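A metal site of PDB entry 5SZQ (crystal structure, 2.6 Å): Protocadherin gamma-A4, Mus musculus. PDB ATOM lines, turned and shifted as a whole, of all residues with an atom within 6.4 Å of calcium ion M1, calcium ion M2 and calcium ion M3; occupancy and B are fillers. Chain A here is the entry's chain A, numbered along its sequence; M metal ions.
OE2 of Glu 226 sits close to N of Tyr 285, at 3.5 Å.
N of Glu 226 lies within hydrogen-bond range of O of Leu 316 (3.0 Å).
The backbone NH (N) of Asp 411 is in hydrogen-bond range of the backbone carbonyl oxygen (O) of Leu 417, at 3.1 Å.
The side-chain amide nitrogen of Asn 364 is in hydrogen-bond range of the side-chain carboxylate of Asp 317 (2.9 Å).
The side-chain carboxylate of Asp 317 lies within hydrogen-bond range of the backbone NH of Ser 361.
Of the 25 residues printed, 4 come within 4 Å of calcium ion M1.
The nearest printed residue that does not touch calcium ion M1 is Asn 227 (4.03 Å).
Six residues have an atom within 4 Å of calcium ion M2: Glu 226, Glu 286, Asp 317, Gln 318, Asp 320 and Asp 360.
Within 4 Å of calcium ion M3: Asn 319, Asn 321, Asp 358, Asp 360, Asn 364 and Asp 411.
The nearest printed residue that does not touch calcium ion M3 is Leu 417 (4.5 Å).
Calcium ion M1 is bound by OD2 of Asp 320 (2.2 Å), OD1 of Asp 284 (2.3 Å) and OE2 of Glu 226 (2.3 Å).
Calcium ion M1 has three donor atoms within binding distance.
Calcium ion M2 is bound by the side-chain carboxylate of Glu 286, the side-chain carboxylate of Glu 226, the backbone carbonyl oxygen of Gln 318, the side-chain carboxylate of Asp 320, the side-chain carboxylate of Asp 317 and the side-chain carboxylate of Asp 360.
Slightly farther from calcium ion M2 lies the side-chain carboxylate (OE1) of Glu 286 (2.9 Å).
Slightly farther from calcium ion M2 lies OE2 of Glu 226 (3.0 Å).
Calcium ion M3 is bound by OD2 of Asp 360 (2.3 Å), OD2 of Asp 411 (2.4 Å), OD1 of Asn 319 (2.4 Å), OD1 of Asp 358 (2.5 Å), O of Asn 321 (2.5 Å) and O of Asn 364 (2.7 Å).
Calcium ion M3 has six donor atoms within binding distance.
Slightly farther from calcium ion M3 lies OD2 of Asp 358 (2.9 Å).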
ATOM      1  N   GLU A 226     -21.128  16.547   7.276  1.00  0.00           N
ATOM      2  CA  GLU A 226     -21.943  16.954   6.129  1.00  0.00           C
ATOM      3  C   GLU A 226     -21.207  16.721   4.817  1.00  0.00           C
ATOM      4  O   GLU A 226     -21.569  15.831   4.045  1.00  0.00           O
ATOM      5  CB  GLU A 226     -22.345  18.419   6.238  1.00  0.00           C
ATOM      6  CG  GLU A 226     -23.146  18.905   5.044  1.00  0.00           C
ATOM      7  CD  GLU A 226     -23.669  20.296   5.238  1.00  0.00           C
ATOM      8  OE1 GLU A 226     -23.456  20.842   6.338  1.00  0.00           O
ATOM      9  OE2 GLU A 226     -24.279  20.846   4.294  1.00  0.00           O
ATOM     10  N   ASN A 227     -20.178  17.515   4.537  1.00  0.00           N
ATOM     11  CA  ASN A 227     -19.331  17.239   3.397  1.00  0.00           C
ATOM     12  C   ASN A 227     -18.346  16.156   3.791  1.00  0.00           C
ATOM     13  O   ASN A 227     -17.837  16.146   4.918  1.00  0.00           O
ATOM     14  CB  ASN A 227     -18.597  18.512   2.945  1.00  0.00           C
ATOM     15  CG  ASN A 227     -19.528  19.720   2.771  1.00  0.00           C
ATOM     16  OD1 ASN A 227     -20.730  19.648   3.049  1.00  0.00           O
ATOM     17  ND2 ASN A 227     -18.963  20.843   2.343  1.00  0.00           N
ATOM     18  N   ASP A 284     -24.932  16.001   1.731  1.00  0.00           N
ATOM     19  CA  ASP A 284     -25.291  17.365   2.113  1.00  0.00           C
ATOM     20  C   ASP A 284     -26.401  17.317   3.159  1.00  0.00           C
ATOM     21  O   ASP A 284     -27.477  16.768   2.903  1.00  0.00           O
ATOM     22  CB  ASP A 284     -25.739  18.166   0.895  1.00  0.00           C
ATOM     23  CG  ASP A 284     -26.058  19.596   1.238  1.00  0.00           C
ATOM     24  OD1 ASP A 284     -25.530  20.101   2.247  1.00  0.00           O
ATOM     25  OD2 ASP A 284     -26.866  20.222   0.518  1.00  0.00           O
ATOM     26  N   TYR A 285     -26.139  17.909   4.327  1.00  0.00           N
ATOM     27  CA  TYR A 285     -27.099  17.803   5.432  1.00  0.00           C
ATOM     28  C   TYR A 285     -28.421  18.470   5.088  1.00  0.00           C
ATOM     29  O   TYR A 285     -29.478  18.019   5.537  1.00  0.00           O
ATOM     30  CB  TYR A 285     -26.529  18.417   6.702  1.00  0.00           C
ATOM     31  CG  TYR A 285     -27.440  18.260   7.913  1.00  0.00           C
ATOM     32  CD1 TYR A 285     -27.370  17.141   8.716  1.00  0.00           C
ATOM     33  CD2 TYR A 285     -28.383  19.227   8.231  1.00  0.00           C
ATOM     34  CE1 TYR A 285     -28.194  16.985   9.809  1.00  0.00           C
ATOM     35  CE2 TYR A 285     -29.225  19.076   9.338  1.00  0.00           C
ATOM     36  CZ  TYR A 285     -29.113  17.949  10.120  1.00  0.00           C
ATOM     37  OH  TYR A 285     -29.935  17.783  11.213  1.00  0.00           O
ATOM     38  N   GLU A 286     -28.393  19.537   4.293  1.00  0.00           N
ATOM     39  CA  GLU A 286     -29.617  20.227   3.910  1.00  0.00           C
ATOM     40  C   GLU A 286     -30.400  19.484   2.847  1.00  0.00           C
ATOM     41  O   GLU A 286     -31.530  19.897   2.533  1.00  0.00           O
ATOM     42  CB  GLU A 286     -29.299  21.639   3.437  1.00  0.00           C
ATOM     43  CG  GLU A 286     -28.845  22.568   4.554  1.00  0.00           C
ATOM     44  CD  GLU A 286     -27.434  22.250   5.044  1.00  0.00           C
ATOM     45  OE1 GLU A 286     -26.581  21.913   4.199  1.00  0.00           O
ATOM     46  OE2 GLU A 286     -27.198  22.338   6.266  1.00  0.00           O
ATOM     47  N   LEU A 316     -24.213  14.665  10.121  1.00  0.00           N
ATOM     48  CA  LEU A 316     -24.053  15.768  11.060  1.00  0.00           C
ATOM     49  C   LEU A 316     -24.002  17.083  10.291  1.00  0.00           C
ATOM     50  O   LEU A 316     -23.279  17.192   9.299  1.00  0.00           O
ATOM     51  CB  LEU A 316     -22.792  15.589  11.906  1.00  0.00           C
ATOM     52  CG  LEU A 316     -22.724  14.350  12.809  1.00  0.00           C
ATOM     53  CD1 LEU A 316     -21.359  14.223  13.455  1.00  0.00           C
ATOM     54  CD2 LEU A 316     -23.812  14.394  13.868  1.00  0.00           C
ATOM     55  N   ASP A 317     -24.776  18.058  10.756  1.00  0.00           N
ATOM     56  CA  ASP A 317     -24.839  19.363  10.103  1.00  0.00           C
ATOM     57  C   ASP A 317     -23.514  20.102  10.241  1.00  0.00           C
ATOM     58  O   ASP A 317     -22.820  19.997  11.256  1.00  0.00           O
ATOM     59  CB  ASP A 317     -25.961  20.200  10.707  1.00  0.00           C
ATOM     60  CG  ASP A 317     -26.049  21.580  10.085  1.00  0.00           C
ATOM     61  OD1 ASP A 317     -26.019  21.685   8.838  1.00  0.00           O
ATOM     62  OD2 ASP A 317     -26.124  22.561  10.842  1.00  0.00           O
ATOM     63  N   GLN A 318     -23.165  20.850   9.201  1.00  0.00           N
ATOM     64  CA  GLN A 318     -21.963  21.670   9.183  1.00  0.00           C
ATOM     65  C   GLN A 318     -22.317  23.084   8.760  1.00  0.00           C
ATOM     66  O   GLN A 318     -23.159  23.283   7.878  1.00  0.00           O
ATOM     67  CB  GLN A 318     -20.904  21.077   8.234  1.00  0.00           C
ATOM     68  CG  GLN A 318     -19.701  21.967   8.020  1.00  0.00           C
ATOM     69  CD  GLN A 318     -18.566  21.265   7.316  1.00  0.00           C
ATOM     70  OE1 GLN A 318     -18.155  20.164   7.705  1.00  0.00           O
ATOM     71  NE2 GLN A 318     -18.036  21.892   6.270  1.00  0.00           N
ATOM     72  N   ASN A 319     -21.681  24.067   9.403  1.00  0.00           N
ATOM     73  CA  ASN A 319     -21.867  25.480   9.063  1.00  0.00           C
ATOM     74  C   ASN A 319     -21.166  25.752   7.738  1.00  0.00           C
ATOM     75  O   ASN A 319     -20.014  26.200   7.680  1.00  0.00           O
ATOM     76  CB  ASN A 319     -21.357  26.395  10.175  1.00  0.00           C
ATOM     77  CG  ASN A 319     -21.681  27.856   9.917  1.00  0.00           C
ATOM     78  OD1 ASN A 319     -22.518  28.171   9.084  1.00  0.00           O
ATOM     79  ND2 ASN A 319     -21.017  28.740  10.643  1.00  0.00           N
ATOM     80  N   ASP A 320     -21.873  25.445   6.647  1.00  0.00           N
ATOM     81  CA  ASP A 320     -21.357  25.626   5.290  1.00  0.00           C
ATOM     82  C   ASP A 320     -22.305  26.473   4.448  1.00  0.00           C
ATOM     83  O   ASP A 320     -22.339  26.336   3.223  1.00  0.00           O
ATOM     84  CB  ASP A 320     -21.115  24.275   4.629  1.00  0.00           C
ATOM     85  CG  ASP A 320     -22.406  23.555   4.267  1.00  0.00           C
ATOM     86  OD1 ASP A 320     -23.396  23.682   5.028  1.00  0.00           O
ATOM     87  OD2 ASP A 320     -22.418  22.861   3.230  1.00  0.00           O
ATOM     88  N   ASN A 321     -23.079  27.358   5.086  1.00  0.00           N
ATOM     89  CA  ASN A 321     -24.018  28.224   4.394  1.00  0.00           C
ATOM     90  C   ASN A 321     -24.019  29.589   5.056  1.00  0.00           C
ATOM     91  O   ASN A 321     -24.272  29.697   6.271  1.00  0.00           O
ATOM     92  CB  ASN A 321     -25.436  27.640   4.395  1.00  0.00           C
ATOM     93  CG  ASN A 321     -25.631  26.593   3.323  1.00  0.00           C
ATOM     94  OD1 ASN A 321     -25.231  26.782   2.175  1.00  0.00           O
ATOM     95  ND2 ASN A 321     -26.245  25.467   3.700  1.00  0.00           N
ATOM     96  N   THR A 322     -23.736  30.622   4.275  1.00  0.00           N
ATOM     97  CA  THR A 322     -23.831  31.984   4.764  1.00  0.00           C
ATOM     98  C   THR A 322     -25.305  32.353   4.954  1.00  0.00           C
ATOM     99  O   THR A 322     -26.178  31.842   4.238  1.00  0.00           O
ATOM    100  CB  THR A 322     -23.184  32.952   3.772  1.00  0.00           C
ATOM    101  OG1 THR A 322     -21.892  32.457   3.394  1.00  0.00           O
ATOM    102  CG2 THR A 322     -23.019  34.341   4.376  1.00  0.00           C
ATOM    103  N   PRO A 323     -25.624  33.183   5.936  1.00  0.00           N
ATOM    104  CA  PRO A 323     -26.993  33.704   6.051  1.00  0.00           C
ATOM    105  C   PRO A 323     -27.397  34.509   4.821  1.00  0.00           C
ATOM    106  O   PRO A 323     -26.586  35.212   4.226  1.00  0.00           O
ATOM    107  CB  PRO A 323     -26.929  34.576   7.310  1.00  0.00           C
ATOM    108  CG  PRO A 323     -25.837  33.976   8.125  1.00  0.00           C
ATOM    109  CD  PRO A 323     -24.828  33.452   7.149  1.00  0.00           C
ATOM    110  N   ASP A 358     -31.102  31.168   7.263  1.00  0.00           N
ATOM    111  CA  ASP A 358     -29.863  30.405   7.148  1.00  0.00           C
ATOM    112  C   ASP A 358     -30.213  28.945   6.860  1.00  0.00           C
ATOM    113  O   ASP A 358     -30.964  28.329   7.624  1.00  0.00           O
ATOM    114  CB  ASP A 358     -29.020  30.518   8.425  1.00  0.00           C
ATOM    115  CG  ASP A 358     -27.627  29.954   8.260  1.00  0.00           C
ATOM    116  OD1 ASP A 358     -26.649  30.693   8.514  1.00  0.00           O
ATOM    117  OD2 ASP A 358     -27.490  28.770   7.893  1.00  0.00           O
ATOM    118  N   LYS A 359     -29.675  28.399   5.762  1.00  0.00           N
ATOM    119  CA  LYS A 359     -30.048  27.053   5.330  1.00  0.00           C
ATOM    120  C   LYS A 359     -29.662  25.986   6.357  1.00  0.00           C
ATOM    121  O   LYS A 359     -30.277  24.913   6.383  1.00  0.00           O
ATOM    122  CB  LYS A 359     -29.410  26.716   3.983  1.00  0.00           C
ATOM    123  CG  LYS A 359     -29.984  27.464   2.808  1.00  0.00           C
ATOM    124  CD  LYS A 359     -29.272  27.096   1.525  1.00  0.00           C
ATOM    125  CE  LYS A 359     -29.808  27.909   0.355  1.00  0.00           C
ATOM    126  NZ  LYS A 359     -29.050  27.650  -0.901  1.00  0.00           N
ATOM    127  N   ASP A 360     -28.655  26.252   7.179  1.00  0.00           N
ATOM    128  CA  ASP A 360     -28.141  25.282   8.137  1.00  0.00           C
ATOM    129  C   ASP A 360     -29.157  25.093   9.272  1.00  0.00           C
ATOM    130  O   ASP A 360     -30.300  25.556   9.215  1.00  0.00           O
ATOM    131  CB  ASP A 360     -26.782  25.724   8.659  1.00  0.00           C
ATOM    132  CG  ASP A 360     -25.808  26.066   7.536  1.00  0.00           C
ATOM    133  OD1 ASP A 360     -25.606  25.216   6.648  1.00  0.00           O
ATOM    134  OD2 ASP A 360     -25.262  27.189   7.532  1.00  0.00           O
ATOM    135  N   SER A 361     -28.739  24.404  10.339  1.00  0.00           N
ATOM    136  CA  SER A 361     -29.618  24.092  11.452  1.00  0.00           C
ATOM    137  C   SER A 361     -28.901  24.405  12.762  1.00  0.00           C
ATOM    138  O   SER A 361     -27.696  24.678  12.784  1.00  0.00           O
ATOM    139  CB  SER A 361     -30.056  22.616  11.408  1.00  0.00           C
ATOM    140  OG  SER A 361     -31.053  22.345  12.371  1.00  0.00           O
ATOM    141  N   GLN A 363     -27.196  25.813  16.008  1.00  0.00           N
ATOM    142  CA  GLN A 363     -26.387  27.015  16.185  1.00  0.00           C
ATOM    143  C   GLN A 363     -25.940  27.594  14.858  1.00  0.00           C
ATOM    144  O   GLN A 363     -25.699  28.800  14.763  1.00  0.00           O
ATOM    145  CB  GLN A 363     -25.166  26.728  17.053  1.00  0.00           C
ATOM    146  CG  GLN A 363     -25.471  26.611  18.533  1.00  0.00           C
ATOM    147  CD  GLN A 363     -24.220  26.692  19.389  1.00  0.00           C
ATOM    148  OE1 GLN A 363     -23.112  26.742  18.874  1.00  0.00           O
ATOM    149  NE2 GLN A 363     -24.392  26.696  20.708  1.00  0.00           N
ATOM    150  N   ASN A 364     -25.819  26.765  13.805  1.00  0.00           N
ATOM    151  CA  ASN A 364     -25.445  27.287  12.502  1.00  0.00           C
ATOM    152  C   ASN A 364     -26.573  28.070  11.835  1.00  0.00           C
ATOM    153  O   ASN A 364     -26.323  28.774  10.840  1.00  0.00           O
ATOM    154  CB  ASN A 364     -24.981  26.132  11.608  1.00  0.00           C
ATOM    155  CG  ASN A 364     -23.966  25.217  12.286  1.00  0.00           C
ATOM    156  OD1 ASN A 364     -23.373  25.564  13.304  1.00  0.00           O
ATOM    157  ND2 ASN A 364     -23.759  24.032  11.709  1.00  0.00           N
ATOM    158  N   ALA A 365     -27.810  27.958  12.344  1.00  0.00           N
ATOM    159  CA  ALA A 365     -28.940  28.745  11.855  1.00  0.00           C
ATOM    160  C   ALA A 365     -29.384  29.798  12.865  1.00  0.00           C
ATOM    161  O   ALA A 365     -30.482  30.341  12.734  1.00  0.00           O
ATOM    162  CB  ALA A 365     -30.110  27.832  11.502  1.00  0.00           C
ATOM    163  N   LEU A 367     -29.115  33.330  14.183  1.00  0.00           N
ATOM    164  CA  LEU A 367     -28.692  34.611  13.637  1.00  0.00           C
ATOM    165  C   LEU A 367     -28.673  35.695  14.705  1.00  0.00           C
ATOM    166  O   LEU A 367     -29.558  35.759  15.565  1.00  0.00           O
ATOM    167  CB  LEU A 367     -29.613  35.046  12.494  1.00  0.00           C
ATOM    168  CG  LEU A 367     -29.483  34.270  11.189  1.00  0.00           C
ATOM    169  CD1 LEU A 367     -28.045  33.828  10.981  1.00  0.00           C
ATOM    170  CD2 LEU A 367     -30.423  33.084  11.164  1.00  0.00           C
ATOM    171  N   ASP A 411     -24.200  34.012  11.789  1.00  0.00           N
ATOM    172  CA  ASP A 411     -24.618  32.753  12.379  1.00  0.00           C
ATOM    173  C   ASP A 411     -23.701  32.421  13.554  1.00  0.00           C
ATOM    174  O   ASP A 411     -22.586  32.935  13.661  1.00  0.00           O
ATOM    175  CB  ASP A 411     -24.612  31.634  11.338  1.00  0.00           C
ATOM    176  CG  ASP A 411     -23.260  31.431  10.684  1.00  0.00           C
ATOM    177  OD1 ASP A 411     -22.346  32.254  10.919  1.00  0.00           O
ATOM    178  OD2 ASP A 411     -23.112  30.453   9.931  1.00  0.00           O
ATOM    179  N   HIS A 412     -24.196  31.568  14.450  1.00  0.00           N
ATOM    180  CA  HIS A 412     -23.468  31.236  15.669  1.00  0.00           C
ATOM    181  C   HIS A 412     -22.754  29.882  15.582  1.00  0.00           C
ATOM    182  O   HIS A 412     -22.509  29.253  16.610  1.00  0.00           O
ATOM    183  CB  HIS A 412     -24.408  31.259  16.873  1.00  0.00           C
ATOM    184  CG  HIS A 412     -24.742  32.650  17.334  1.00  0.00           C
ATOM    185  ND1 HIS A 412     -26.040  33.076  17.518  1.00  0.00           N
ATOM    186  CD2 HIS A 412     -23.947  33.695  17.646  1.00  0.00           C
ATOM    187  CE1 HIS A 412     -26.033  34.336  17.928  1.00  0.00           C
ATOM    188  NE2 HIS A 412     -24.773  34.730  18.020  1.00  0.00           N
ATOM    189  N   GLY A 413     -22.430  29.439  14.376  1.00  0.00           N
ATOM    190  CA  GLY A 413     -21.703  28.197  14.195  1.00  0.00           C
ATOM    191  C   GLY A 413     -20.193  28.387  14.307  1.00  0.00           C
ATOM    192  O   GLY A 413     -19.694  29.474  14.611  1.00  0.00           O
ATOM    193  N   LEU A 417     -20.208  32.788   9.982  1.00  0.00           N
ATOM    194  CA  LEU A 417     -20.277  33.441   8.685  1.00  0.00           C
ATOM    195  C   LEU A 417     -21.185  34.659   8.760  1.00  0.00           C
ATOM    196  O   LEU A 417     -22.208  34.641   9.464  1.00  0.00           O
ATOM    197  CB  LEU A 417     -20.786  32.472   7.600  1.00  0.00           C
ATOM    198  CG  LEU A 417     -20.124  31.089   7.552  1.00  0.00           C
ATOM    199  CD1 LEU A 417     -20.865  30.157   6.582  1.00  0.00           C
ATOM    200  CD2 LEU A 417     -18.642  31.181   7.185  1.00  0.00           C
HETATM  201 CA    CA M   1     -24.012  21.834   2.208  1.00  0.00          CA
HETATM  202 CA    CA M   2     -25.096  22.574   6.604  1.00  0.00          CA
HETATM  203 CA    CA M   3     -24.715  29.135   8.704  1.00  0.00          CA
